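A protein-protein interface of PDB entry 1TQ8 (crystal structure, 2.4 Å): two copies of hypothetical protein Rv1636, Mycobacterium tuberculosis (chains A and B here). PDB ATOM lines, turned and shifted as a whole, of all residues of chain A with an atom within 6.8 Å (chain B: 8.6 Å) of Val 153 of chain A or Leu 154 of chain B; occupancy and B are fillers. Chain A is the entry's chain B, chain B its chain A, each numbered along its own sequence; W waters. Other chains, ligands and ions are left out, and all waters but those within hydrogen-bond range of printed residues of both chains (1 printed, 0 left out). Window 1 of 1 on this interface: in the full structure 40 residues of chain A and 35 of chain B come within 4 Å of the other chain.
The backbone carbonyl oxygen (O) of Asp 152 of chain B is in hydrogen-bond range of the backbone NH (N) of Leu 123 of chain A (2.8 Å).
The side-chain hydroxyl of Tyr 17 of chain B is in hydrogen-bond range of the side-chain carboxylate of Asp 152 of chain A (2.7 Å).
N of Leu 154 of chain B lies within hydrogen-bond range of O of Leu 123 of chain A (2.8 Å).
O of Leu 154 of chain A sits at hydrogen-bond distance from N of Val 125 of chain B (3.1 Å).
OD1 of Asp 152 of chain A is in hydrogen-bond range of ND1 of His 157 of chain B, at 2.6 Å.
The backbone carbonyl oxygen of Asp 152 of chain A is in hydrogen-bond range of the backbone NH of Leu 123 of chain B, at 2.8 Å.
N of Asp 152 of chain A is in hydrogen-bond range of O of Asp 121 of chain B, 3.3 Å away.
N of Val 125 of chain A sits at hydrogen-bond distance from O of Leu 154 of chain B (3.1 Å).
The side-chain hydroxyl (OH) of Tyr 17 of chain B sits close to the guanidinium group (NE) of Arg 36 of chain A (3.2 Å).
N of Val 156 of chain B is in hydrogen-bond range of O of Val 125 of chain A, at 3.0 Å.
The backbone carbonyl oxygen (O) of Val 153 of chain B lies within hydrogen-bond range of the backbone NH (N) of Ile 155 of chain A (2.8 Å).
N of Ile 155 of chain B sits at hydrogen-bond distance from O of Val 153 of chain A (2.7 Å).
O of Leu 123 of chain B sits at hydrogen-bond distance from N of Leu 154 of chain A, 2.7 Å away.
The backbone carbonyl oxygen (O) of Leu 122 of chain B lies within hydrogen-bond range of the backbone NH (N) of Val 21 of chain B (3.0 Å).
OG of Ser 146 of chain B is in hydrogen-bond range of O of Val 151 of chain B (3.0 Å).
NE of Arg 36 of chain A is in salt-bridge range of OD2 of Asp 152 of chain A.
The backbone carbonyl oxygen (O) of Val 151 of chain A lies within hydrogen-bond range of the side-chain hydroxyl (OG) of Ser 146 of chain A (2.9 Å).
O of Val 21 of chain B sits at hydrogen-bond distance from N of Val 124 of chain B, at 2.8 Å.
Arg 36 of chain A touches Leu 154 of chain B (CG to CD2, 3.95 Å).
CD1 of Ile 40 of chain A touches CD2 of Leu 154 of chain B, at 3.8 Å.
Leu 154 of chain B touches Val 124 of chain A (O to CA, 3.4 Å).
O of Val 125 of chain A touches CA of Ile 155 of chain B, 3.7 Å away.
Gly 126 of chain A touches Val 156 of chain B.
OG of Ser 146 of chain A touches CG2 of Ile 155 of chain B, 3.9 Å away.
Ile 155 of chain B touches Asp 152 of chain A (O to CA, 3.1 Å).
CA of Val 153 of chain A touches O of Leu 123 of chain B, 3.5 Å away.
CB of Leu 154 of chain A touches CD1 of Leu 122 of chain B, 3.9 Å away.
Val 153 of chain B touches Leu 154 of chain A.
Ala 37 of chain A touches none of the printed residues of chain B.
Of the printed residues of chain B, Val 125 of chain A touches Leu 154 (3.1 Å), Ile 155 (3.7 Å) and Val 156 (3.0 Å).
Val 153 of chain A touches just these residues of chain B: Leu 123, Val 153, Leu 154 and Ile 155.
Val 21 of chain B touches none of the printed residues of chain A.
Of the printed residues of chain A, Ser 146 of chain B touches Ile 155 (3.9 Å).
Printed residues of chain A within 4 Å of Val 153 of chain B: Leu 123, Val 153, Leu 154 and Ile 155.
Of the printed residues of chain A, Val 156 of chain B touches Ala 33 (3.9 Å), Val 124 (3.8 Å), Val 125 (3.0 Å), Gly 126 (3.7 Å) and Asp 152 (3.4 Å).
Of the 20 printed residues of chain A, 17 touch a printed residue of chain B.
Hydrophobic or aromatic side chains of chain A that line the printed part of chain B: Ile 40, Leu 122, Leu 123, Val 124, Pro 142, Val 145, Val 151, Leu 154 and Ile 155.
Hydrophobic or aromatic side chains of chain B within 4 Å of the printed part of chain A: Tyr 17, Ile 40, Leu 122, Leu 123, Pro 142, Val 151, Leu 154, Ile 155, Val 156 and His 157.
Among the printed residues, 47 pairs touch across the chains.
Among the printed residues, no Asp or Glu carboxylate lies within 4 Å of a Lys or Arg side-chain nitrogen of the other chain.
Leu 123 of chain A touches Asp 152 of chain B, and with the chains exchanged Asp 152 of chain A touches Leu 123 of chain B.
Val 125 of chain A touches Leu 154 of chain B, and with the chains exchanged Leu 154 of chain A touches Val 125 of chain B.
Pro 142 of chain B touches its own counterpart, Pro 142 of chain A.
Val 153 of chain B touches its own counterpart, Val 153 of chain A.
Positions printed for both chains: 40, 122, 123, 124, 125, 142, 146, 151, 152, 153, 154 and 155.
Water W1 lies within hydrogen-bond range of the backbone carbonyl oxygen (O) of Asp 121 of chain B, a ring nitrogen (ND1) of His 157 of chain B and the side-chain carboxylate (OD1) of Asp 152 of chain A.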
ATOM      1  N   ALA A  33      30.329  -3.525  21.102  1.00  0.00           N
ATOM      2  CA  ALA A  33      28.996  -4.047  20.867  1.00  0.00           C
ATOM      3  C   ALA A  33      28.176  -3.934  22.144  1.00  0.00           C
ATOM      4  O   ALA A  33      26.955  -3.764  22.093  1.00  0.00           O
ATOM      5  CB  ALA A  33      29.066  -5.496  20.423  1.00  0.00           C
ATOM      6  N   ARG A  36      26.861  -0.353  22.415  1.00  0.00           N
ATOM      7  CA  ARG A  36      25.740  -0.159  21.508  1.00  0.00           C
ATOM      8  C   ARG A  36      24.494  -0.881  22.010  1.00  0.00           C
ATOM      9  O   ARG A  36      23.394  -0.340  21.965  1.00  0.00           O
ATOM     10  CB  ARG A  36      26.090  -0.661  20.098  1.00  0.00           C
ATOM     11  CG  ARG A  36      24.911  -0.660  19.107  1.00  0.00           C
ATOM     12  CD  ARG A  36      24.363   0.740  18.893  1.00  0.00           C
ATOM     13  NE  ARG A  36      25.421   1.655  18.475  1.00  0.00           N
ATOM     14  CZ  ARG A  36      25.292   2.976  18.446  1.00  0.00           C
ATOM     15  NH1 ARG A  36      24.146   3.529  18.814  1.00  0.00           N
ATOM     16  NH2 ARG A  36      26.301   3.742  18.052  1.00  0.00           N
ATOM     17  N   ALA A  37      24.661  -2.109  22.483  1.00  0.00           N
ATOM     18  CA  ALA A  37      23.523  -2.869  22.975  1.00  0.00           C
ATOM     19  C   ALA A  37      22.878  -2.143  24.158  1.00  0.00           C
ATOM     20  O   ALA A  37      21.647  -2.062  24.258  1.00  0.00           O
ATOM     21  CB  ALA A  37      23.967  -4.262  23.390  1.00  0.00           C
ATOM     22  N   ILE A  40      20.898   0.924  23.319  1.00  0.00           N
ATOM     23  CA  ILE A  40      19.580   0.548  22.834  1.00  0.00           C
ATOM     24  C   ILE A  40      18.696   0.061  23.977  1.00  0.00           C
ATOM     25  O   ILE A  40      17.501   0.369  24.027  1.00  0.00           O
ATOM     26  CB  ILE A  40      19.675  -0.564  21.766  1.00  0.00           C
ATOM     27  CG1 ILE A  40      20.467  -0.061  20.556  1.00  0.00           C
ATOM     28  CG2 ILE A  40      18.284  -0.996  21.340  1.00  0.00           C
ATOM     29  CD1 ILE A  40      20.739  -1.123  19.514  1.00  0.00           C
ATOM     30  N   LEU A 122      16.211  -8.852  19.953  1.00  0.00           N
ATOM     31  CA  LEU A 122      17.404  -8.337  19.294  1.00  0.00           C
ATOM     32  C   LEU A 122      18.696  -9.002  19.784  1.00  0.00           C
ATOM     33  O   LEU A 122      18.917  -9.112  20.992  1.00  0.00           O
ATOM     34  CB  LEU A 122      17.516  -6.821  19.506  1.00  0.00           C
ATOM     35  CG  LEU A 122      18.767  -6.160  18.903  1.00  0.00           C
ATOM     36  CD1 LEU A 122      18.759  -6.386  17.409  1.00  0.00           C
ATOM     37  CD2 LEU A 122      18.797  -4.674  19.210  1.00  0.00           C
ATOM     38  N   LEU A 123      19.540  -9.456  18.854  1.00  0.00           N
ATOM     39  CA  LEU A 123      20.825 -10.052  19.232  1.00  0.00           C
ATOM     40  C   LEU A 123      21.887  -9.104  18.695  1.00  0.00           C
ATOM     41  O   LEU A 123      21.747  -8.561  17.598  1.00  0.00           O
ATOM     42  CB  LEU A 123      21.029 -11.438  18.617  1.00  0.00           C
ATOM     43  CG  LEU A 123      19.977 -12.526  18.839  1.00  0.00           C
ATOM     44  CD1 LEU A 123      20.522 -13.828  18.271  1.00  0.00           C
ATOM     45  CD2 LEU A 123      19.651 -12.683  20.328  1.00  0.00           C
ATOM     46  N   VAL A 124      22.948  -8.913  19.469  1.00  0.00           N
ATOM     47  CA  VAL A 124      24.019  -8.004  19.095  1.00  0.00           C
ATOM     48  C   VAL A 124      25.390  -8.659  19.260  1.00  0.00           C
ATOM     49  O   VAL A 124      25.676  -9.260  20.300  1.00  0.00           O
ATOM     50  CB  VAL A 124      23.977  -6.732  19.995  1.00  0.00           C
ATOM     51  CG1 VAL A 124      25.018  -5.737  19.563  1.00  0.00           C
ATOM     52  CG2 VAL A 124      22.597  -6.115  19.965  1.00  0.00           C
ATOM     53  N   VAL A 125      26.234  -8.560  18.235  1.00  0.00           N
ATOM     54  CA  VAL A 125      27.589  -9.098  18.333  1.00  0.00           C
ATOM     55  C   VAL A 125      28.540  -8.112  17.706  1.00  0.00           C
ATOM     56  O   VAL A 125      28.146  -7.308  16.865  1.00  0.00           O
ATOM     57  CB  VAL A 125      27.779 -10.457  17.611  1.00  0.00           C
ATOM     58  CG1 VAL A 125      26.832 -11.507  18.195  1.00  0.00           C
ATOM     59  CG2 VAL A 125      27.561 -10.297  16.124  1.00  0.00           C
ATOM     60  N   GLY A 126      29.796  -8.180  18.131  1.00  0.00           N
ATOM     61  CA  GLY A 126      30.814  -7.301  17.598  1.00  0.00           C
ATOM     62  C   GLY A 126      31.413  -7.991  16.395  1.00  0.00           C
ATOM     63  O   GLY A 126      31.662  -9.192  16.431  1.00  0.00           O
ATOM     64  N   VAL A 141      28.572 -12.190   4.004  1.00  0.00           N
ATOM     65  CA  VAL A 141      28.523 -10.861   3.413  1.00  0.00           C
ATOM     66  C   VAL A 141      28.106  -9.791   4.427  1.00  0.00           C
ATOM     67  O   VAL A 141      28.618  -8.679   4.403  1.00  0.00           O
ATOM     68  CB  VAL A 141      27.573 -10.856   2.190  1.00  0.00           C
ATOM     69  CG1 VAL A 141      27.558  -9.478   1.523  1.00  0.00           C
ATOM     70  CG2 VAL A 141      28.045 -11.903   1.182  1.00  0.00           C
ATOM     71  N   PRO A 142      27.173 -10.112   5.334  1.00  0.00           N
ATOM     72  CA  PRO A 142      26.819  -9.052   6.278  1.00  0.00           C
ATOM     73  C   PRO A 142      28.010  -8.612   7.132  1.00  0.00           C
ATOM     74  O   PRO A 142      28.205  -7.417   7.370  1.00  0.00           O
ATOM     75  CB  PRO A 142      25.651  -9.651   7.079  1.00  0.00           C
ATOM     76  CG  PRO A 142      25.638 -11.104   6.734  1.00  0.00           C
ATOM     77  CD  PRO A 142      26.209 -11.225   5.377  1.00  0.00           C
ATOM     78  N   ALA A 143      28.829  -9.566   7.557  1.00  0.00           N
ATOM     79  CA  ALA A 143      30.018  -9.251   8.353  1.00  0.00           C
ATOM     80  C   ALA A 143      31.012  -8.481   7.504  1.00  0.00           C
ATOM     81  O   ALA A 143      31.687  -7.550   7.958  1.00  0.00           O
ATOM     82  CB  ALA A 143      30.684 -10.538   8.842  1.00  0.00           C
ATOM     83  N   VAL A 145      30.393  -6.597   4.734  1.00  0.00           N
ATOM     84  CA  VAL A 145      29.965  -5.244   4.415  1.00  0.00           C
ATOM     85  C   VAL A 145      30.184  -4.324   5.607  1.00  0.00           C
ATOM     86  O   VAL A 145      30.580  -3.167   5.450  1.00  0.00           O
ATOM     87  CB  VAL A 145      28.482  -5.231   3.982  1.00  0.00           C
ATOM     88  CG1 VAL A 145      27.924  -3.799   3.980  1.00  0.00           C
ATOM     89  CG2 VAL A 145      28.367  -5.850   2.592  1.00  0.00           C
ATOM     90  N   SER A 146      29.927  -4.851   6.801  1.00  0.00           N
ATOM     91  CA  SER A 146      30.105  -4.087   8.022  1.00  0.00           C
ATOM     92  C   SER A 146      31.546  -3.611   8.153  1.00  0.00           C
ATOM     93  O   SER A 146      31.804  -2.494   8.602  1.00  0.00           O
ATOM     94  CB  SER A 146      29.739  -4.943   9.231  1.00  0.00           C
ATOM     95  OG  SER A 146      30.218  -4.342  10.423  1.00  0.00           O
ATOM     96  N   ARG A 147      32.486  -4.465   7.762  1.00  0.00           N
ATOM     97  CA  ARG A 147      33.896  -4.109   7.834  1.00  0.00           C
ATOM     98  C   ARG A 147      34.284  -3.161   6.696  1.00  0.00           C
ATOM     99  O   ARG A 147      34.993  -2.182   6.911  1.00  0.00           O
ATOM    100  CB  ARG A 147      34.774  -5.366   7.763  1.00  0.00           C
ATOM    101  CG  ARG A 147      36.218  -5.132   8.174  1.00  0.00           C
ATOM    102  CD  ARG A 147      37.145  -6.264   7.749  1.00  0.00           C
ATOM    103  NE  ARG A 147      37.579  -6.069   6.369  1.00  0.00           N
ATOM    104  CZ  ARG A 147      37.118  -6.753   5.328  1.00  0.00           C
ATOM    105  NH1 ARG A 147      36.207  -7.703   5.500  1.00  0.00           N
ATOM    106  NH2 ARG A 147      37.546  -6.458   4.109  1.00  0.00           N
ATOM    107  N   VAL A 151      30.463   0.163   9.198  1.00  0.00           N
ATOM    108  CA  VAL A 151      29.118   0.538   9.570  1.00  0.00           C
ATOM    109  C   VAL A 151      28.452  -0.639  10.266  1.00  0.00           C
ATOM    110  O   VAL A 151      28.879  -1.777  10.107  1.00  0.00           O
ATOM    111  CB  VAL A 151      28.315   0.880   8.301  1.00  0.00           C
ATOM    112  CG1 VAL A 151      28.094  -0.401   7.493  1.00  0.00           C
ATOM    113  CG2 VAL A 151      27.004   1.528   8.656  1.00  0.00           C
ATOM    114  N   ASP A 152      27.390  -0.373  11.019  1.00  0.00           N
ATOM    115  CA  ASP A 152      26.681  -1.445  11.694  1.00  0.00           C
ATOM    116  C   ASP A 152      25.594  -2.009  10.775  1.00  0.00           C
ATOM    117  O   ASP A 152      24.988  -1.272   9.987  1.00  0.00           O
ATOM    118  CB  ASP A 152      26.069  -0.929  12.995  1.00  0.00           C
ATOM    119  CG  ASP A 152      27.118  -0.446  13.986  1.00  0.00           C
ATOM    120  OD1 ASP A 152      28.328  -0.689  13.744  1.00  0.00           O
ATOM    121  OD2 ASP A 152      26.724   0.164  15.012  1.00  0.00           O
ATOM    122  N   VAL A 153      25.340  -3.311  10.879  1.00  0.00           N
ATOM    123  CA  VAL A 153      24.339  -3.952  10.037  1.00  0.00           C
ATOM    124  C   VAL A 153      23.230  -4.611  10.830  1.00  0.00           C
ATOM    125  O   VAL A 153      23.475  -5.393  11.744  1.00  0.00           O
ATOM    126  CB  VAL A 153      24.990  -4.993   9.084  1.00  0.00           C
ATOM    127  CG1 VAL A 153      23.912  -5.742   8.289  1.00  0.00           C
ATOM    128  CG2 VAL A 153      25.929  -4.276   8.122  1.00  0.00           C
ATOM    129  N   LEU A 154      22.000  -4.283  10.456  1.00  0.00           N
ATOM    130  CA  LEU A 154      20.821  -4.806  11.121  1.00  0.00           C
ATOM    131  C   LEU A 154      19.972  -5.661  10.193  1.00  0.00           C
ATOM    132  O   LEU A 154      19.583  -5.224   9.113  1.00  0.00           O
ATOM    133  CB  LEU A 154      19.989  -3.644  11.653  1.00  0.00           C
ATOM    134  CG  LEU A 154      18.673  -4.004  12.329  1.00  0.00           C
ATOM    135  CD1 LEU A 154      18.928  -4.848  13.580  1.00  0.00           C
ATOM    136  CD2 LEU A 154      17.962  -2.710  12.685  1.00  0.00           C
ATOM    137  N   ILE A 155      19.704  -6.887  10.627  1.00  0.00           N
ATOM    138  CA  ILE A 155      18.893  -7.828   9.868  1.00  0.00           C
ATOM    139  C   ILE A 155      17.575  -7.978  10.625  1.00  0.00           C
ATOM    140  O   ILE A 155      17.539  -8.487  11.747  1.00  0.00           O
ATOM    141  CB  ILE A 155      19.589  -9.209   9.769  1.00  0.00           C
ATOM    142  CG1 ILE A 155      20.968  -9.047   9.141  1.00  0.00           C
ATOM    143  CG2 ILE A 155      18.750 -10.173   8.952  1.00  0.00           C
ATOM    144  CD1 ILE A 155      21.752 -10.345   9.052  1.00  0.00           C
ATOM    145  N   TYR B  17      21.948   6.549  16.320  1.00  0.00           N
ATOM    146  CA  TYR B  17      22.309   6.522  14.913  1.00  0.00           C
ATOM    147  C   TYR B  17      21.777   7.778  14.235  1.00  0.00           C
ATOM    148  O   TYR B  17      20.620   8.138  14.423  1.00  0.00           O
ATOM    149  CB  TYR B  17      21.703   5.289  14.250  1.00  0.00           C
ATOM    150  CG  TYR B  17      22.346   4.002  14.682  1.00  0.00           C
ATOM    151  CD1 TYR B  17      21.589   2.978  15.242  1.00  0.00           C
ATOM    152  CD2 TYR B  17      23.723   3.798  14.515  1.00  0.00           C
ATOM    153  CE1 TYR B  17      22.185   1.783  15.626  1.00  0.00           C
ATOM    154  CE2 TYR B  17      24.323   2.606  14.893  1.00  0.00           C
ATOM    155  CZ  TYR B  17      23.546   1.602  15.448  1.00  0.00           C
ATOM    156  OH  TYR B  17      24.130   0.409  15.815  1.00  0.00           O
ATOM    157  N   VAL B  21      20.335   3.702   6.525  1.00  0.00           N
ATOM    158  CA  VAL B  21      20.020   3.302   5.161  1.00  0.00           C
ATOM    159  C   VAL B  21      19.333   1.946   5.248  1.00  0.00           C
ATOM    160  O   VAL B  21      19.836   1.038   5.902  1.00  0.00           O
ATOM    161  CB  VAL B  21      21.290   3.169   4.281  1.00  0.00           C
ATOM    162  CG1 VAL B  21      20.894   2.804   2.854  1.00  0.00           C
ATOM    163  CG2 VAL B  21      22.064   4.472   4.281  1.00  0.00           C
ATOM    164  N   ILE B  40      13.814   3.632  14.236  1.00  0.00           N
ATOM    165  CA  ILE B  40      15.138   3.956  14.744  1.00  0.00           C
ATOM    166  C   ILE B  40      15.575   5.347  14.320  1.00  0.00           C
ATOM    167  O   ILE B  40      16.261   6.042  15.063  1.00  0.00           O
ATOM    168  CB  ILE B  40      16.189   2.940  14.233  1.00  0.00           C
ATOM    169  CG1 ILE B  40      15.803   1.535  14.688  1.00  0.00           C
ATOM    170  CG2 ILE B  40      17.583   3.327  14.718  1.00  0.00           C
ATOM    171  CD1 ILE B  40      16.700   0.441  14.178  1.00  0.00           C
ATOM    172  N   LEU B 111      25.669  -0.252  -2.422  1.00  0.00           N
ATOM    173  CA  LEU B 111      25.313   0.049  -1.039  1.00  0.00           C
ATOM    174  C   LEU B 111      26.527   0.544  -0.235  1.00  0.00           C
ATOM    175  O   LEU B 111      26.419   1.490   0.546  1.00  0.00           O
ATOM    176  CB  LEU B 111      24.683  -1.173  -0.366  1.00  0.00           C
ATOM    177  CG  LEU B 111      24.160  -0.967   1.058  1.00  0.00           C
ATOM    178  CD1 LEU B 111      23.032   0.054   1.027  1.00  0.00           C
ATOM    179  CD2 LEU B 111      23.667  -2.302   1.661  1.00  0.00           C
ATOM    180  N   ASP B 121      25.639   5.109   9.323  1.00  0.00           N
ATOM    181  CA  ASP B 121      26.150   4.464  10.525  1.00  0.00           C
ATOM    182  C   ASP B 121      25.360   3.190  10.829  1.00  0.00           C
ATOM    183  O   ASP B 121      25.711   2.421  11.720  1.00  0.00           O
ATOM    184  CB  ASP B 121      26.158   5.428  11.727  1.00  0.00           C
ATOM    185  CG  ASP B 121      24.820   6.099  11.968  1.00  0.00           C
ATOM    186  OD1 ASP B 121      24.816   7.173  12.605  1.00  0.00           O
ATOM    187  OD2 ASP B 121      23.775   5.565  11.541  1.00  0.00           O
ATOM    188  N   LEU B 122      24.319   2.948  10.045  1.00  0.00           N
ATOM    189  CA  LEU B 122      23.503   1.759  10.219  1.00  0.00           C
ATOM    190  C   LEU B 122      22.819   1.327   8.921  1.00  0.00           C
ATOM    191  O   LEU B 122      22.112   2.121   8.295  1.00  0.00           O
ATOM    192  CB  LEU B 122      22.434   2.012  11.288  1.00  0.00           C
ATOM    193  CG  LEU B 122      21.352   0.932  11.396  1.00  0.00           C
ATOM    194  CD1 LEU B 122      22.027  -0.359  11.842  1.00  0.00           C
ATOM    195  CD2 LEU B 122      20.258   1.334  12.392  1.00  0.00           C
ATOM    196  N   LEU B 123      23.030   0.078   8.513  1.00  0.00           N
ATOM    197  CA  LEU B 123      22.377  -0.440   7.316  1.00  0.00           C
ATOM    198  C   LEU B 123      21.333  -1.441   7.791  1.00  0.00           C
ATOM    199  O   LEU B 123      21.591  -2.244   8.685  1.00  0.00           O
ATOM    200  CB  LEU B 123      23.369  -1.139   6.392  1.00  0.00           C
ATOM    201  CG  LEU B 123      24.569  -0.310   5.954  1.00  0.00           C
ATOM    202  CD1 LEU B 123      25.394  -1.156   5.015  1.00  0.00           C
ATOM    203  CD2 LEU B 123      24.129   0.989   5.279  1.00  0.00           C
ATOM    204  N   VAL B 124      20.158  -1.394   7.179  1.00  0.00           N
ATOM    205  CA  VAL B 124      19.063  -2.260   7.562  1.00  0.00           C
ATOM    206  C   VAL B 124      18.448  -2.993   6.378  1.00  0.00           C
ATOM    207  O   VAL B 124      18.188  -2.383   5.339  1.00  0.00           O
ATOM    208  CB  VAL B 124      17.925  -1.429   8.188  1.00  0.00           C
ATOM    209  CG1 VAL B 124      16.813  -2.341   8.652  1.00  0.00           C
ATOM    210  CG2 VAL B 124      18.456  -0.567   9.318  1.00  0.00           C
ATOM    211  N   VAL B 125      18.198  -4.291   6.536  1.00  0.00           N
ATOM    212  CA  VAL B 125      17.533  -5.059   5.491  1.00  0.00           C
ATOM    213  C   VAL B 125      16.596  -6.070   6.116  1.00  0.00           C
ATOM    214  O   VAL B 125      16.771  -6.472   7.262  1.00  0.00           O
ATOM    215  CB  VAL B 125      18.525  -5.823   4.575  1.00  0.00           C
ATOM    216  CG1 VAL B 125      19.429  -4.830   3.844  1.00  0.00           C
ATOM    217  CG2 VAL B 125      19.361  -6.813   5.391  1.00  0.00           C
ATOM    218  N   PRO B 142      24.281 -15.419  10.278  1.00  0.00           N
ATOM    219  CA  PRO B 142      23.474 -14.365  10.895  1.00  0.00           C
ATOM    220  C   PRO B 142      22.063 -14.316  10.325  1.00  0.00           C
ATOM    221  O   PRO B 142      21.110 -14.052  11.054  1.00  0.00           O
ATOM    222  CB  PRO B 142      24.290 -13.094  10.643  1.00  0.00           C
ATOM    223  CG  PRO B 142      25.143 -13.435   9.477  1.00  0.00           C
ATOM    224  CD  PRO B 142      25.522 -14.869   9.711  1.00  0.00           C
ATOM    225  N   SER B 146      18.562 -15.249  12.531  1.00  0.00           N
ATOM    226  CA  SER B 146      17.443 -14.326  12.482  1.00  0.00           C
ATOM    227  C   SER B 146      16.139 -15.073  12.208  1.00  0.00           C
ATOM    228  O   SER B 146      15.116 -14.794  12.824  1.00  0.00           O
ATOM    229  CB  SER B 146      17.673 -13.278  11.394  1.00  0.00           C
ATOM    230  OG  SER B 146      16.539 -12.436  11.243  1.00  0.00           O
ATOM    231  N   VAL B 151      14.233 -13.384  15.368  1.00  0.00           N
ATOM    232  CA  VAL B 151      14.737 -12.194  16.037  1.00  0.00           C
ATOM    233  C   VAL B 151      15.615 -11.339  15.113  1.00  0.00           C
ATOM    234  O   VAL B 151      16.133 -11.820  14.115  1.00  0.00           O
ATOM    235  CB  VAL B 151      15.533 -12.607  17.311  1.00  0.00           C
ATOM    236  CG1 VAL B 151      16.788 -13.370  16.917  1.00  0.00           C
ATOM    237  CG2 VAL B 151      15.876 -11.386  18.151  1.00  0.00           C
ATOM    238  N   ASP B 152      15.764 -10.063  15.442  1.00  0.00           N
ATOM    239  CA  ASP B 152      16.587  -9.165  14.650  1.00  0.00           C
ATOM    240  C   ASP B 152      18.034  -9.327  15.106  1.00  0.00           C
ATOM    241  O   ASP B 152      18.302  -9.538  16.296  1.00  0.00           O
ATOM    242  CB  ASP B 152      16.149  -7.710  14.857  1.00  0.00           C
ATOM    243  CG  ASP B 152      14.804  -7.396  14.225  1.00  0.00           C
ATOM    244  OD1 ASP B 152      14.186  -8.301  13.623  1.00  0.00           O
ATOM    245  OD2 ASP B 152      14.362  -6.229  14.327  1.00  0.00           O
ATOM    246  N   VAL B 153      18.960  -9.200  14.159  1.00  0.00           N
ATOM    247  CA  VAL B 153      20.382  -9.334  14.443  1.00  0.00           C
ATOM    248  C   VAL B 153      21.135  -8.059  14.091  1.00  0.00           C
ATOM    249  O   VAL B 153      20.926  -7.477  13.027  1.00  0.00           O
ATOM    250  CB  VAL B 153      20.985 -10.524  13.662  1.00  0.00           C
ATOM    251  CG1 VAL B 153      22.502 -10.595  13.881  1.00  0.00           C
ATOM    252  CG2 VAL B 153      20.325 -11.822  14.126  1.00  0.00           C
ATOM    253  N   LEU B 154      22.021  -7.636  14.986  1.00  0.00           N
ATOM    254  CA  LEU B 154      22.784  -6.416  14.785  1.00  0.00           C
ATOM    255  C   LEU B 154      24.283  -6.647  14.858  1.00  0.00           C
ATOM    256  O   LEU B 154      24.788  -7.134  15.866  1.00  0.00           O
ATOM    257  CB  LEU B 154      22.381  -5.393  15.844  1.00  0.00           C
ATOM    258  CG  LEU B 154      23.176  -4.089  15.854  1.00  0.00           C
ATOM    259  CD1 LEU B 154      22.955  -3.352  14.537  1.00  0.00           C
ATOM    260  CD2 LEU B 154      22.725  -3.228  17.044  1.00  0.00           C
ATOM    261  N   ILE B 155      24.988  -6.298  13.787  1.00  0.00           N
ATOM    262  CA  ILE B 155      26.435  -6.460  13.738  1.00  0.00           C
ATOM    263  C   ILE B 155      27.067  -5.093  13.950  1.00  0.00           C
ATOM    264  O   ILE B 155      26.818  -4.161  13.185  1.00  0.00           O
ATOM    265  CB  ILE B 155      26.899  -7.037  12.376  1.00  0.00           C
ATOM    266  CG1 ILE B 155      26.243  -8.400  12.134  1.00  0.00           C
ATOM    267  CG2 ILE B 155      28.409  -7.184  12.361  1.00  0.00           C
ATOM    268  CD1 ILE B 155      26.545  -8.987  10.785  1.00  0.00           C
ATOM    269  N   VAL B 156      27.879  -4.979  14.996  1.00  0.00           N
ATOM    270  CA  VAL B 156      28.531  -3.720  15.341  1.00  0.00           C
ATOM    271  C   VAL B 156      29.937  -3.701  14.781  1.00  0.00           C
ATOM    272  O   VAL B 156      30.766  -4.536  15.139  1.00  0.00           O
ATOM    273  CB  VAL B 156      28.599  -3.547  16.876  1.00  0.00           C
ATOM    274  CG1 VAL B 156      29.359  -2.280  17.234  1.00  0.00           C
ATOM    275  CG2 VAL B 156      27.202  -3.514  17.444  1.00  0.00           C
ATOM    276  N   HIS B 157      30.211  -2.753  13.897  1.00  0.00           N
ATOM    277  CA  HIS B 157      31.532  -2.675  13.300  1.00  0.00           C
ATOM    278  C   HIS B 157      32.546  -2.296  14.364  1.00  0.00           C
ATOM    279  O   HIS B 157      32.167  -1.941  15.471  1.00  0.00           O
ATOM    280  CB  HIS B 157      31.551  -1.648  12.157  1.00  0.00           C
ATOM    281  CG  HIS B 157      31.638  -0.223  12.608  1.00  0.00           C
ATOM    282  ND1 HIS B 157      30.578   0.450  13.180  1.00  0.00           N
ATOM    283  CD2 HIS B 157      32.659   0.667  12.551  1.00  0.00           C
ATOM    284  CE1 HIS B 157      30.942   1.692  13.449  1.00  0.00           C
ATOM    285  NE2 HIS B 157      32.200   1.849  13.076  1.00  0.00           N
HETATM  286  O   HOH W   1      28.168   2.705  13.192  1.00  0.00           O
